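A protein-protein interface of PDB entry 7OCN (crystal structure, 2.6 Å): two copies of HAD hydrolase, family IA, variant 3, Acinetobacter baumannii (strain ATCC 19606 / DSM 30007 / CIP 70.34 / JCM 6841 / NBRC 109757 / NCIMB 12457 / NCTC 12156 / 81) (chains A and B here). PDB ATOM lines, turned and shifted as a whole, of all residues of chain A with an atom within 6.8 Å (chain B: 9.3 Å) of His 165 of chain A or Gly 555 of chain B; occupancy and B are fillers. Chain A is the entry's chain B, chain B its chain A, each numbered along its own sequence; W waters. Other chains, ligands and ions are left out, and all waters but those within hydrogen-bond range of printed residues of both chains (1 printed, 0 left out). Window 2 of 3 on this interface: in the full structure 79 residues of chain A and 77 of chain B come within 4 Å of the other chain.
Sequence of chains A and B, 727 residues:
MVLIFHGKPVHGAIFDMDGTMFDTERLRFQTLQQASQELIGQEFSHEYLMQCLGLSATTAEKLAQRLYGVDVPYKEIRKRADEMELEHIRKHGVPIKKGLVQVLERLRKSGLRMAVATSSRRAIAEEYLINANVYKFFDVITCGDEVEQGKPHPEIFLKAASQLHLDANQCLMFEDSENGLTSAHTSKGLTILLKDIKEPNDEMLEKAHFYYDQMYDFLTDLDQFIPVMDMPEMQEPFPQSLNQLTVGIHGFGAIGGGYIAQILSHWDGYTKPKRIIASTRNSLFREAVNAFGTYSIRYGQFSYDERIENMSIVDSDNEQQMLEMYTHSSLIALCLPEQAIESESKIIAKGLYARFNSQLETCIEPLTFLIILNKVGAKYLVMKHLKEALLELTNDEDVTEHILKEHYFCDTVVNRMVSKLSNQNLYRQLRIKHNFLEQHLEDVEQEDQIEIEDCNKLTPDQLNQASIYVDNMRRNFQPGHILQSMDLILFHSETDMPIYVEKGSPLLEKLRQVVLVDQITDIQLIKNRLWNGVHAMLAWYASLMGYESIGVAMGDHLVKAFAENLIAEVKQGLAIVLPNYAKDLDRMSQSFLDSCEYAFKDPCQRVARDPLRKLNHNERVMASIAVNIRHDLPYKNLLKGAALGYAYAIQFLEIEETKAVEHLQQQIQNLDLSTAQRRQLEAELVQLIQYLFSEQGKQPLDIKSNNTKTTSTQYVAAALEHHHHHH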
ATOM      1  N   ARG A 113     -28.790 -17.471   5.735  1.00  0.00           N
ATOM      2  CA  ARG A 113     -27.369 -17.080   5.934  1.00  0.00           C
ATOM      3  C   ARG A 113     -27.053 -17.205   7.429  1.00  0.00           C
ATOM      4  O   ARG A 113     -27.477 -16.322   8.198  1.00  0.00           O
ATOM      5  CB  ARG A 113     -27.124 -15.671   5.382  1.00  0.00           C
ATOM      6  CG  ARG A 113     -27.875 -15.370   4.092  1.00  0.00           C
ATOM      7  CD  ARG A 113     -27.247 -14.268   3.258  1.00  0.00           C
ATOM      8  NE  ARG A 113     -26.239 -14.774   2.334  1.00  0.00           N
ATOM      9  CZ  ARG A 113     -26.495 -15.445   1.210  1.00  0.00           C
ATOM     10  NH1 ARG A 113     -25.493 -15.857   0.449  1.00  0.00           N
ATOM     11  NH2 ARG A 113     -27.739 -15.712   0.849  1.00  0.00           N
ATOM     12  N   VAL A 140     -20.026 -16.965   8.322  1.00  0.00           N
ATOM     13  CA  VAL A 140     -19.072 -16.166   9.154  1.00  0.00           C
ATOM     14  C   VAL A 140     -19.341 -16.486  10.628  1.00  0.00           C
ATOM     15  O   VAL A 140     -20.481 -16.861  10.945  1.00  0.00           O
ATOM     16  CB  VAL A 140     -19.206 -14.654   8.881  1.00  0.00           C
ATOM     17  CG1 VAL A 140     -18.073 -13.866   9.524  1.00  0.00           C
ATOM     18  CG2 VAL A 140     -19.288 -14.350   7.390  1.00  0.00           C
ATOM     19  N   ALA A 160     -21.980  -9.952  13.903  1.00  0.00           N
ATOM     20  CA  ALA A 160     -22.309 -11.278  13.325  1.00  0.00           C
ATOM     21  C   ALA A 160     -23.368 -11.118  12.228  1.00  0.00           C
ATOM     22  O   ALA A 160     -23.187 -11.705  11.145  1.00  0.00           O
ATOM     23  CB  ALA A 160     -22.779 -12.214  14.412  1.00  0.00           C
ATOM     24  N   ALA A 161     -24.424 -10.345  12.504  1.00  0.00           N
ATOM     25  CA  ALA A 161     -25.547 -10.065  11.576  1.00  0.00           C
ATOM     26  C   ALA A 161     -25.050  -9.239  10.382  1.00  0.00           C
ATOM     27  O   ALA A 161     -25.475  -9.533   9.248  1.00  0.00           O
ATOM     28  CB  ALA A 161     -26.658  -9.354  12.310  1.00  0.00           C
ATOM     29  N   SER A 162     -24.189  -8.248  10.635  1.00  0.00           N
ATOM     30  CA  SER A 162     -23.623  -7.321   9.618  1.00  0.00           C
ATOM     31  C   SER A 162     -22.735  -8.091   8.631  1.00  0.00           C
ATOM     32  O   SER A 162     -22.793  -7.782   7.424  1.00  0.00           O
ATOM     33  CB  SER A 162     -22.864  -6.193  10.271  1.00  0.00           C
ATOM     34  OG  SER A 162     -22.454  -5.234   9.308  1.00  0.00           O
ATOM     35  N   GLN A 163     -21.954  -9.058   9.124  1.00  0.00           N
ATOM     36  CA  GLN A 163     -21.002  -9.869   8.315  1.00  0.00           C
ATOM     37  C   GLN A 163     -21.766 -10.854   7.419  1.00  0.00           C
ATOM     38  O   GLN A 163     -21.170 -11.315   6.427  1.00  0.00           O
ATOM     39  CB  GLN A 163     -20.010 -10.599   9.224  1.00  0.00           C
ATOM     40  CG  GLN A 163     -18.920  -9.690   9.776  1.00  0.00           C
ATOM     41  CD  GLN A 163     -17.953 -10.407  10.686  1.00  0.00           C
ATOM     42  OE1 GLN A 163     -16.753 -10.145  10.673  1.00  0.00           O
ATOM     43  NE2 GLN A 163     -18.470 -11.318  11.495  1.00  0.00           N
ATOM     44  N   LEU A 164     -23.026 -11.164   7.752  1.00  0.00           N
ATOM     45  CA  LEU A 164     -23.943 -11.984   6.910  1.00  0.00           C
ATOM     46  C   LEU A 164     -24.580 -11.110   5.821  1.00  0.00           C
ATOM     47  O   LEU A 164     -25.219 -11.680   4.914  1.00  0.00           O
ATOM     48  CB  LEU A 164     -25.025 -12.619   7.792  1.00  0.00           C
ATOM     49  CG  LEU A 164     -24.555 -13.723   8.737  1.00  0.00           C
ATOM     50  CD1 LEU A 164     -25.655 -14.086   9.724  1.00  0.00           C
ATOM     51  CD2 LEU A 164     -24.101 -14.951   7.960  1.00  0.00           C
ATOM     52  N   HIS A 165     -24.421  -9.784   5.915  1.00  0.00           N
ATOM     53  CA  HIS A 165     -24.951  -8.771   4.960  1.00  0.00           C
ATOM     54  C   HIS A 165     -26.484  -8.754   5.033  1.00  0.00           C
ATOM     55  O   HIS A 165     -27.130  -8.722   3.966  1.00  0.00           O
ATOM     56  CB  HIS A 165     -24.415  -9.028   3.542  1.00  0.00           C
ATOM     57  CG  HIS A 165     -22.963  -9.372   3.493  1.00  0.00           C
ATOM     58  ND1 HIS A 165     -22.021  -8.717   4.263  1.00  0.00           N
ATOM     59  CD2 HIS A 165     -22.289 -10.294   2.772  1.00  0.00           C
ATOM     60  CE1 HIS A 165     -20.830  -9.222   4.020  1.00  0.00           C
ATOM     61  NE2 HIS A 165     -20.967 -10.192   3.109  1.00  0.00           N
ATOM     62  N   LEU A 166     -27.032  -8.774   6.254  1.00  0.00           N
ATOM     63  CA  LEU A 166     -28.492  -8.713   6.543  1.00  0.00           C
ATOM     64  C   LEU A 166     -28.720  -7.891   7.817  1.00  0.00           C
ATOM     65  O   LEU A 166     -27.794  -7.819   8.649  1.00  0.00           O
ATOM     66  CB  LEU A 166     -29.036 -10.137   6.711  1.00  0.00           C
ATOM     67  CG  LEU A 166     -29.183 -10.954   5.427  1.00  0.00           C
ATOM     68  CD1 LEU A 166     -29.431 -12.420   5.748  1.00  0.00           C
ATOM     69  CD2 LEU A 166     -30.300 -10.404   4.552  1.00  0.00           C
ATOM     70  N   ASP A 167     -29.910  -7.298   7.956  1.00  0.00           N
ATOM     71  CA  ASP A 167     -30.337  -6.553   9.173  1.00  0.00           C
ATOM     72  C   ASP A 167     -30.570  -7.561  10.305  1.00  0.00           C
ATOM     73  O   ASP A 167     -30.999  -8.694  10.008  1.00  0.00           O
ATOM     74  CB  ASP A 167     -31.581  -5.703   8.900  1.00  0.00           C
ATOM     75  CG  ASP A 167     -31.367  -4.581   7.897  1.00  0.00           C
ATOM     76  OD1 ASP A 167     -30.207  -4.151   7.731  1.00  0.00           O
ATOM     77  OD2 ASP A 167     -32.365  -4.143   7.291  1.00  0.00           O
ATOM     78  N   GLN A 170     -33.871  -9.522  10.877  1.00  0.00           N
ATOM     79  CA  GLN A 170     -34.152 -10.620   9.910  1.00  0.00           C
ATOM     80  C   GLN A 170     -33.530 -11.937  10.396  1.00  0.00           C
ATOM     81  O   GLN A 170     -33.830 -12.980   9.781  1.00  0.00           O
ATOM     82  CB  GLN A 170     -33.601 -10.272   8.526  1.00  0.00           C
ATOM     83  CG  GLN A 170     -34.233  -9.034   7.904  1.00  0.00           C
ATOM     84  CD  GLN A 170     -33.629  -8.707   6.559  1.00  0.00           C
ATOM     85  OE1 GLN A 170     -32.481  -8.281   6.460  1.00  0.00           O
ATOM     86  NE2 GLN A 170     -34.407  -8.904   5.506  1.00  0.00           N
ATOM     87  N   TYR B 547     -12.445  -1.321   2.776  1.00  0.00           N
ATOM     88  CA  TYR B 547     -12.824  -2.694   3.204  1.00  0.00           C
ATOM     89  C   TYR B 547     -11.678  -3.655   2.863  1.00  0.00           C
ATOM     90  O   TYR B 547     -11.132  -3.562   1.744  1.00  0.00           O
ATOM     91  CB  TYR B 547     -14.141  -3.119   2.549  1.00  0.00           C
ATOM     92  CG  TYR B 547     -15.336  -2.282   2.935  1.00  0.00           C
ATOM     93  CD1 TYR B 547     -15.847  -2.316   4.223  1.00  0.00           C
ATOM     94  CD2 TYR B 547     -15.963  -1.458   2.014  1.00  0.00           C
ATOM     95  CE1 TYR B 547     -16.944  -1.552   4.587  1.00  0.00           C
ATOM     96  CE2 TYR B 547     -17.063  -0.688   2.360  1.00  0.00           C
ATOM     97  CZ  TYR B 547     -17.555  -0.735   3.653  1.00  0.00           C
ATOM     98  OH  TYR B 547     -18.636   0.021   4.001  1.00  0.00           O
ATOM     99  N   SER B 549     -11.507  -7.097   2.455  1.00  0.00           N
ATOM    100  CA  SER B 549     -11.889  -8.044   1.373  1.00  0.00           C
ATOM    101  C   SER B 549     -13.110  -7.508   0.617  1.00  0.00           C
ATOM    102  O   SER B 549     -13.867  -6.706   1.200  1.00  0.00           O
ATOM    103  CB  SER B 549     -12.152  -9.420   1.929  1.00  0.00           C
ATOM    104  OG  SER B 549     -13.315  -9.425   2.745  1.00  0.00           O
ATOM    105  N   ILE B 550     -13.282  -7.945  -0.635  1.00  0.00           N
ATOM    106  CA  ILE B 550     -14.443  -7.600  -1.511  1.00  0.00           C
ATOM    107  C   ILE B 550     -15.719  -8.209  -0.913  1.00  0.00           C
ATOM    108  O   ILE B 550     -16.799  -7.621  -1.116  1.00  0.00           O
ATOM    109  CB  ILE B 550     -14.195  -8.065  -2.962  1.00  0.00           C
ATOM    110  CG1 ILE B 550     -15.160  -7.399  -3.948  1.00  0.00           C
ATOM    111  CG2 ILE B 550     -14.238  -9.583  -3.076  1.00  0.00           C
ATOM    112  CD1 ILE B 550     -14.717  -7.491  -5.389  1.00  0.00           C
ATOM    113  N   GLY B 551     -15.591  -9.340  -0.208  1.00  0.00           N
ATOM    114  CA  GLY B 551     -16.696 -10.039   0.480  1.00  0.00           C
ATOM    115  C   GLY B 551     -17.281  -9.209   1.612  1.00  0.00           C
ATOM    116  O   GLY B 551     -18.522  -9.148   1.710  1.00  0.00           O
ATOM    117  N   VAL B 552     -16.423  -8.604   2.442  1.00  0.00           N
ATOM    118  CA  VAL B 552     -16.818  -7.708   3.572  1.00  0.00           C
ATOM    119  C   VAL B 552     -17.587  -6.506   3.007  1.00  0.00           C
ATOM    120  O   VAL B 552     -18.592  -6.111   3.628  1.00  0.00           O
ATOM    121  CB  VAL B 552     -15.593  -7.260   4.396  1.00  0.00           C
ATOM    122  CG1 VAL B 552     -15.881  -6.031   5.248  1.00  0.00           C
ATOM    123  CG2 VAL B 552     -15.058  -8.388   5.264  1.00  0.00           C
ATOM    124  N   ALA B 553     -17.132  -5.964   1.873  1.00  0.00           N
ATOM    125  CA  ALA B 553     -17.658  -4.733   1.232  1.00  0.00           C
ATOM    126  C   ALA B 553     -19.130  -4.910   0.834  1.00  0.00           C
ATOM    127  O   ALA B 553     -19.860  -3.902   0.847  1.00  0.00           O
ATOM    128  CB  ALA B 553     -16.808  -4.372   0.037  1.00  0.00           C
ATOM    129  N   MET B 554     -19.549  -6.137   0.501  1.00  0.00           N
ATOM    130  CA  MET B 554     -20.934  -6.461   0.050  1.00  0.00           C
ATOM    131  C   MET B 554     -21.938  -6.224   1.190  1.00  0.00           C
ATOM    132  O   MET B 554     -23.143  -6.125   0.890  1.00  0.00           O
ATOM    133  CB  MET B 554     -21.036  -7.912  -0.430  1.00  0.00           C
ATOM    134  CG  MET B 554     -20.259  -8.184  -1.708  1.00  0.00           C
ATOM    135  SD  MET B 554     -21.027  -7.463  -3.185  1.00  0.00           S
ATOM    136  CE  MET B 554     -22.312  -8.668  -3.511  1.00  0.00           C
ATOM    137  N   GLY B 555     -21.464  -6.151   2.441  1.00  0.00           N
ATOM    138  CA  GLY B 555     -22.259  -5.723   3.610  1.00  0.00           C
ATOM    139  C   GLY B 555     -22.809  -4.317   3.430  1.00  0.00           C
ATOM    140  O   GLY B 555     -23.956  -4.073   3.855  1.00  0.00           O
ATOM    141  N   ASP B 556     -22.015  -3.427   2.825  1.00  0.00           N
ATOM    142  CA  ASP B 556     -22.425  -2.054   2.426  1.00  0.00           C
ATOM    143  C   ASP B 556     -23.405  -2.168   1.252  1.00  0.00           C
ATOM    144  O   ASP B 556     -23.018  -2.756   0.222  1.00  0.00           O
ATOM    145  CB  ASP B 556     -21.201  -1.203   2.067  1.00  0.00           C
ATOM    146  CG  ASP B 556     -21.467   0.289   1.949  1.00  0.00           C
ATOM    147  OD1 ASP B 556     -22.651   0.681   1.923  1.00  0.00           O
ATOM    148  OD2 ASP B 556     -20.481   1.049   1.882  1.00  0.00           O
ATOM    149  N   HIS B 557     -24.623  -1.638   1.412  1.00  0.00           N
ATOM    150  CA  HIS B 557     -25.716  -1.674   0.399  1.00  0.00           C
ATOM    151  C   HIS B 557     -25.261  -0.983  -0.893  1.00  0.00           C
ATOM    152  O   HIS B 557     -25.647  -1.461  -1.977  1.00  0.00           O
ATOM    153  CB  HIS B 557     -27.005  -1.050   0.956  1.00  0.00           C
ATOM    154  CG  HIS B 557     -27.793  -1.965   1.836  1.00  0.00           C
ATOM    155  ND1 HIS B 557     -28.006  -1.700   3.176  1.00  0.00           N
ATOM    156  CD2 HIS B 557     -28.420  -3.133   1.575  1.00  0.00           C
ATOM    157  CE1 HIS B 557     -28.732  -2.668   3.702  1.00  0.00           C
ATOM    158  NE2 HIS B 557     -28.998  -3.560   2.741  1.00  0.00           N
ATOM    159  N   LEU B 558     -24.475   0.095  -0.777  1.00  0.00           N
ATOM    160  CA  LEU B 558     -23.934   0.883  -1.919  1.00  0.00           C
ATOM    161  C   LEU B 558     -23.104  -0.025  -2.835  1.00  0.00           C
ATOM    162  O   LEU B 558     -23.329   0.012  -4.061  1.00  0.00           O
ATOM    163  CB  LEU B 558     -23.083   2.036  -1.375  1.00  0.00           C
ATOM    164  CG  LEU B 558     -23.854   3.158  -0.683  1.00  0.00           C
ATOM    165  CD1 LEU B 558     -22.916   4.043   0.124  1.00  0.00           C
ATOM    166  CD2 LEU B 558     -24.636   3.984  -1.694  1.00  0.00           C
ATOM    167  N   VAL B 559     -22.186  -0.806  -2.253  1.00  0.00           N
ATOM    168  CA  VAL B 559     -21.234  -1.703  -2.977  1.00  0.00           C
ATOM    169  C   VAL B 559     -22.030  -2.813  -3.675  1.00  0.00           C
ATOM    170  O   VAL B 559     -21.777  -3.058  -4.871  1.00  0.00           O
ATOM    171  CB  VAL B 559     -20.173  -2.292  -2.024  1.00  0.00           C
ATOM    172  CG1 VAL B 559     -19.278  -3.304  -2.725  1.00  0.00           C
ATOM    173  CG2 VAL B 559     -19.333  -1.208  -1.365  1.00  0.00           C
ATOM    174  N   LYS B 560     -22.948  -3.456  -2.946  1.00  0.00           N
ATOM    175  CA  LYS B 560     -23.774  -4.595  -3.434  1.00  0.00           C
ATOM    176  C   LYS B 560     -24.708  -4.111  -4.551  1.00  0.00           C
ATOM    177  O   LYS B 560     -24.833  -4.829  -5.561  1.00  0.00           O
ATOM    178  CB  LYS B 560     -24.562  -5.213  -2.275  1.00  0.00           C
ATOM    179  CG  LYS B 560     -25.250  -6.534  -2.590  1.00  0.00           C
ATOM    180  CD  LYS B 560     -25.651  -7.309  -1.355  1.00  0.00           C
ATOM    181  CE  LYS B 560     -26.313  -8.632  -1.676  1.00  0.00           C
ATOM    182  NZ  LYS B 560     -26.616  -9.402  -0.448  1.00  0.00           N
ATOM    183  N   ALA B 561     -25.333  -2.942  -4.369  1.00  0.00           N
ATOM    184  CA  ALA B 561     -26.242  -2.297  -5.347  1.00  0.00           C
ATOM    185  C   ALA B 561     -25.474  -1.968  -6.633  1.00  0.00           C
ATOM    186  O   ALA B 561     -26.035  -2.185  -7.726  1.00  0.00           O
ATOM    187  CB  ALA B 561     -26.861  -1.058  -4.746  1.00  0.00           C
ATOM    188  N   LEU B 593     -22.248 -12.877  -8.878  1.00  0.00           N
ATOM    189  CA  LEU B 593     -22.890 -12.183  -7.725  1.00  0.00           C
ATOM    190  C   LEU B 593     -22.917 -13.110  -6.502  1.00  0.00           C
ATOM    191  O   LEU B 593     -22.738 -12.598  -5.378  1.00  0.00           O
ATOM    192  CB  LEU B 593     -24.305 -11.741  -8.116  1.00  0.00           C
ATOM    193  CG  LEU B 593     -24.383 -10.623  -9.155  1.00  0.00           C
ATOM    194  CD1 LEU B 593     -25.820 -10.394  -9.597  1.00  0.00           C
ATOM    195  CD2 LEU B 593     -23.780  -9.334  -8.619  1.00  0.00           C
ATOM    196  N   ASP B 594     -23.130 -14.413  -6.715  1.00  0.00           N
ATOM    197  CA  ASP B 594     -23.154 -15.453  -5.649  1.00  0.00           C
ATOM    198  C   ASP B 594     -21.760 -15.584  -5.024  1.00  0.00           C
ATOM    199  O   ASP B 594     -21.672 -15.605  -3.779  1.00  0.00           O
ATOM    200  CB  ASP B 594     -23.636 -16.803  -6.190  1.00  0.00           C
ATOM    201  CG  ASP B 594     -25.137 -16.884  -6.417  1.00  0.00           C
ATOM    202  OD1 ASP B 594     -25.755 -15.825  -6.646  1.00  0.00           O
ATOM    203  OD2 ASP B 594     -25.676 -18.006  -6.357  1.00  0.00           O
ATOM    204  N   SER B 595     -20.717 -15.666  -5.858  1.00  0.00           N
ATOM    205  CA  SER B 595     -19.303 -15.880  -5.449  1.00  0.00           C
ATOM    206  C   SER B 595     -18.768 -14.657  -4.692  1.00  0.00           C
ATOM    207  O   SER B 595     -18.026 -14.857  -3.711  1.00  0.00           O
ATOM    208  CB  SER B 595     -18.438 -16.215  -6.641  1.00  0.00           C
ATOM    209  OG  SER B 595     -18.393 -15.135  -7.561  1.00  0.00           O
ATOM    210  N   CYS B 596     -19.137 -13.447  -5.129  1.00  0.00           N
ATOM    211  CA  CYS B 596     -18.703 -12.146  -4.544  1.00  0.00           C
ATOM    212  C   CYS B 596     -19.227 -11.976  -3.111  1.00  0.00           C
ATOM    213  O   CYS B 596     -18.572 -11.253  -2.336  1.00  0.00           O
ATOM    214  CB  CYS B 596     -19.180 -10.968  -5.387  1.00  0.00           C
ATOM    215  SG  CYS B 596     -18.190 -10.701  -6.880  1.00  0.00           S
ATOM    216  N   GLU B 597     -20.360 -12.607  -2.781  1.00  0.00           N
ATOM    217  CA  GLU B 597     -21.100 -12.427  -1.500  1.00  0.00           C
ATOM    218  C   GLU B 597     -20.157 -12.645  -0.309  1.00  0.00           C
ATOM    219  O   GLU B 597     -20.072 -11.736   0.542  1.00  0.00           O
ATOM    220  CB  GLU B 597     -22.297 -13.380  -1.434  1.00  0.00           C
ATOM    221  CG  GLU B 597     -23.342 -12.977  -0.407  1.00  0.00           C
ATOM    222  CD  GLU B 597     -24.051 -11.661  -0.683  1.00  0.00           C
ATOM    223  OE1 GLU B 597     -24.565 -11.057   0.279  1.00  0.00           O
ATOM    224  OE2 GLU B 597     -24.093 -11.244  -1.859  1.00  0.00           O
ATOM    225  N   TYR B 598     -19.482 -13.799  -0.252  1.00  0.00           N
ATOM    226  CA  TYR B 598     -18.557 -14.194   0.846  1.00  0.00           C
ATOM    227  C   TYR B 598     -17.179 -14.536   0.267  1.00  0.00           C
ATOM    228  O   TYR B 598     -16.673 -15.648   0.522  1.00  0.00           O
ATOM    229  CB  TYR B 598     -19.142 -15.360   1.649  1.00  0.00           C
ATOM    230  CG  TYR B 598     -20.441 -15.056   2.355  1.00  0.00           C
ATOM    231  CD1 TYR B 598     -20.556 -13.966   3.204  1.00  0.00           C
ATOM    232  CD2 TYR B 598     -21.553 -15.866   2.189  1.00  0.00           C
ATOM    233  CE1 TYR B 598     -21.744 -13.681   3.859  1.00  0.00           C
ATOM    234  CE2 TYR B 598     -22.748 -15.597   2.838  1.00  0.00           C
ATOM    235  CZ  TYR B 598     -22.844 -14.500   3.677  1.00  0.00           C
ATOM    236  OH  TYR B 598     -24.017 -14.226   4.318  1.00  0.00           O
ATOM    237  N   ALA B 599     -16.590 -13.596  -0.480  1.00  0.00           N
ATOM    238  CA  ALA B 599     -15.222 -13.682  -1.047  1.00  0.00           C
ATOM    239  C   ALA B 599     -14.248 -12.952  -0.113  1.00  0.00           C
ATOM    240  O   ALA B 599     -13.818 -11.831  -0.453  1.00  0.00           O
ATOM    241  CB  ALA B 599     -15.201 -13.108  -2.444  1.00  0.00           C
ATOM    242  N   PHE B 600     -13.922 -13.576   1.023  1.00  0.00           N
ATOM    243  CA  PHE B 600     -13.091 -13.003   2.115  1.00  0.00           C
ATOM    244  C   PHE B 600     -11.603 -13.251   1.838  1.00  0.00           C
ATOM    245  O   PHE B 600     -10.810 -12.295   1.953  1.00  0.00           O
ATOM    246  CB  PHE B 600     -13.487 -13.600   3.468  1.00  0.00           C
ATOM    247  CG  PHE B 600     -14.892 -13.283   3.918  1.00  0.00           C
ATOM    248  CD1 PHE B 600     -15.250 -11.987   4.254  1.00  0.00           C
ATOM    249  CD2 PHE B 600     -15.852 -14.279   4.020  1.00  0.00           C
ATOM    250  CE1 PHE B 600     -16.539 -11.691   4.671  1.00  0.00           C
ATOM    251  CE2 PHE B 600     -17.140 -13.982   4.438  1.00  0.00           C
ATOM    252  CZ  PHE B 600     -17.481 -12.689   4.763  1.00  0.00           C
HETATM  253  O   HOH W   1     -23.743 -17.155  -1.790  1.00  0.00           O
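NE2 of His 165 of chain A is in hydrogen-bond range of O of Glu 597 of chain B.
O of Gly 551 of chain B sits at hydrogen-bond distance from NE2 of His 165 of chain A, at 3.0 Å.
N of Gly 555 of chain B lies close to ND1 of His 165 of chain A (3.2 Å).
OH of Tyr 598 of chain B is in hydrogen-bond range of NE of Arg 113 of chain A.
OH of Tyr 598 of chain B is in hydrogen-bond range of O of Leu 164 of chain A.
The side-chain carboxylate of Glu 597 of chain B lies within salt-bridge range of the side-chain amino group of Lys 560 of chain B, 2.7 Å away.
N of Val 552 of chain B sits at hydrogen-bond distance from OG of Ser 549 of chain B (3.2 Å).
A ring nitrogen (ND1) of His 165 of chain A sits at hydrogen-bond distance from the backbone carbonyl oxygen of Ser 162 of chain A (3.4 Å).
O of Gln 163 of chain A lies close to ND1 of His 165 of chain A, 3.5 Å away.
The backbone NH (N) of Gly 551 of chain B lies within hydrogen-bond range of the backbone carbonyl oxygen (O) of Ala 599 of chain B.
Arg 113 of chain A touches Glu 597 of chain B.
Phe 600 of chain B touches Val 140 of chain A (CZ to CG2, 3.6 Å).
Gln 163 of chain A touches Tyr 598 of chain B.
His 165 of chain A touches Val 552 of chain B.
Met 554 of chain B touches His 165 of chain A.
Tyr 598 of chain B touches His 165 of chain A.
His 165 of chain A touches just these residues of chain B: Gly 551, Val 552, Met 554, Gly 555, Glu 597 and Tyr 598.
No residue of chain B comes within 4 Å of Leu 166 of chain A.
Printed residues of chain A within 4 Å of Val 552 of chain B: His 165.
Of the printed residues of chain A, Glu 597 of chain B touches Arg 113 (3.7 Å) and His 165 (3.1 Å).
Val 559 of chain B touches none of the printed residues of chain A.
Ser 549 of chain B touches none of the printed residues of chain A.
Of the 11 printed residues of chain A, 5 touch a printed residue of chain B.
Printed residues of chain A that touch a printed residue of chain B: Arg 113, Val 140, Gln 163, Leu 164 and His 165.
Hydrophobic or aromatic side chains of chain A that line the printed part of chain B: Val 140, Leu 164 and His 165.
Hydrophobic or aromatic side chains of chain B within 4 Å of the printed part of chain A: Tyr 598 and Phe 600.
Among the printed residues, 11 pairs touch across the chains.
No position is printed for both chains.
Of the 11 pairs that touch across the chains among the printed residues, none has its exchanged pair printed and touching as well.
Water W1 bridges NH1 of Arg 113 of chain A and O of Asp 594 of chain B.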
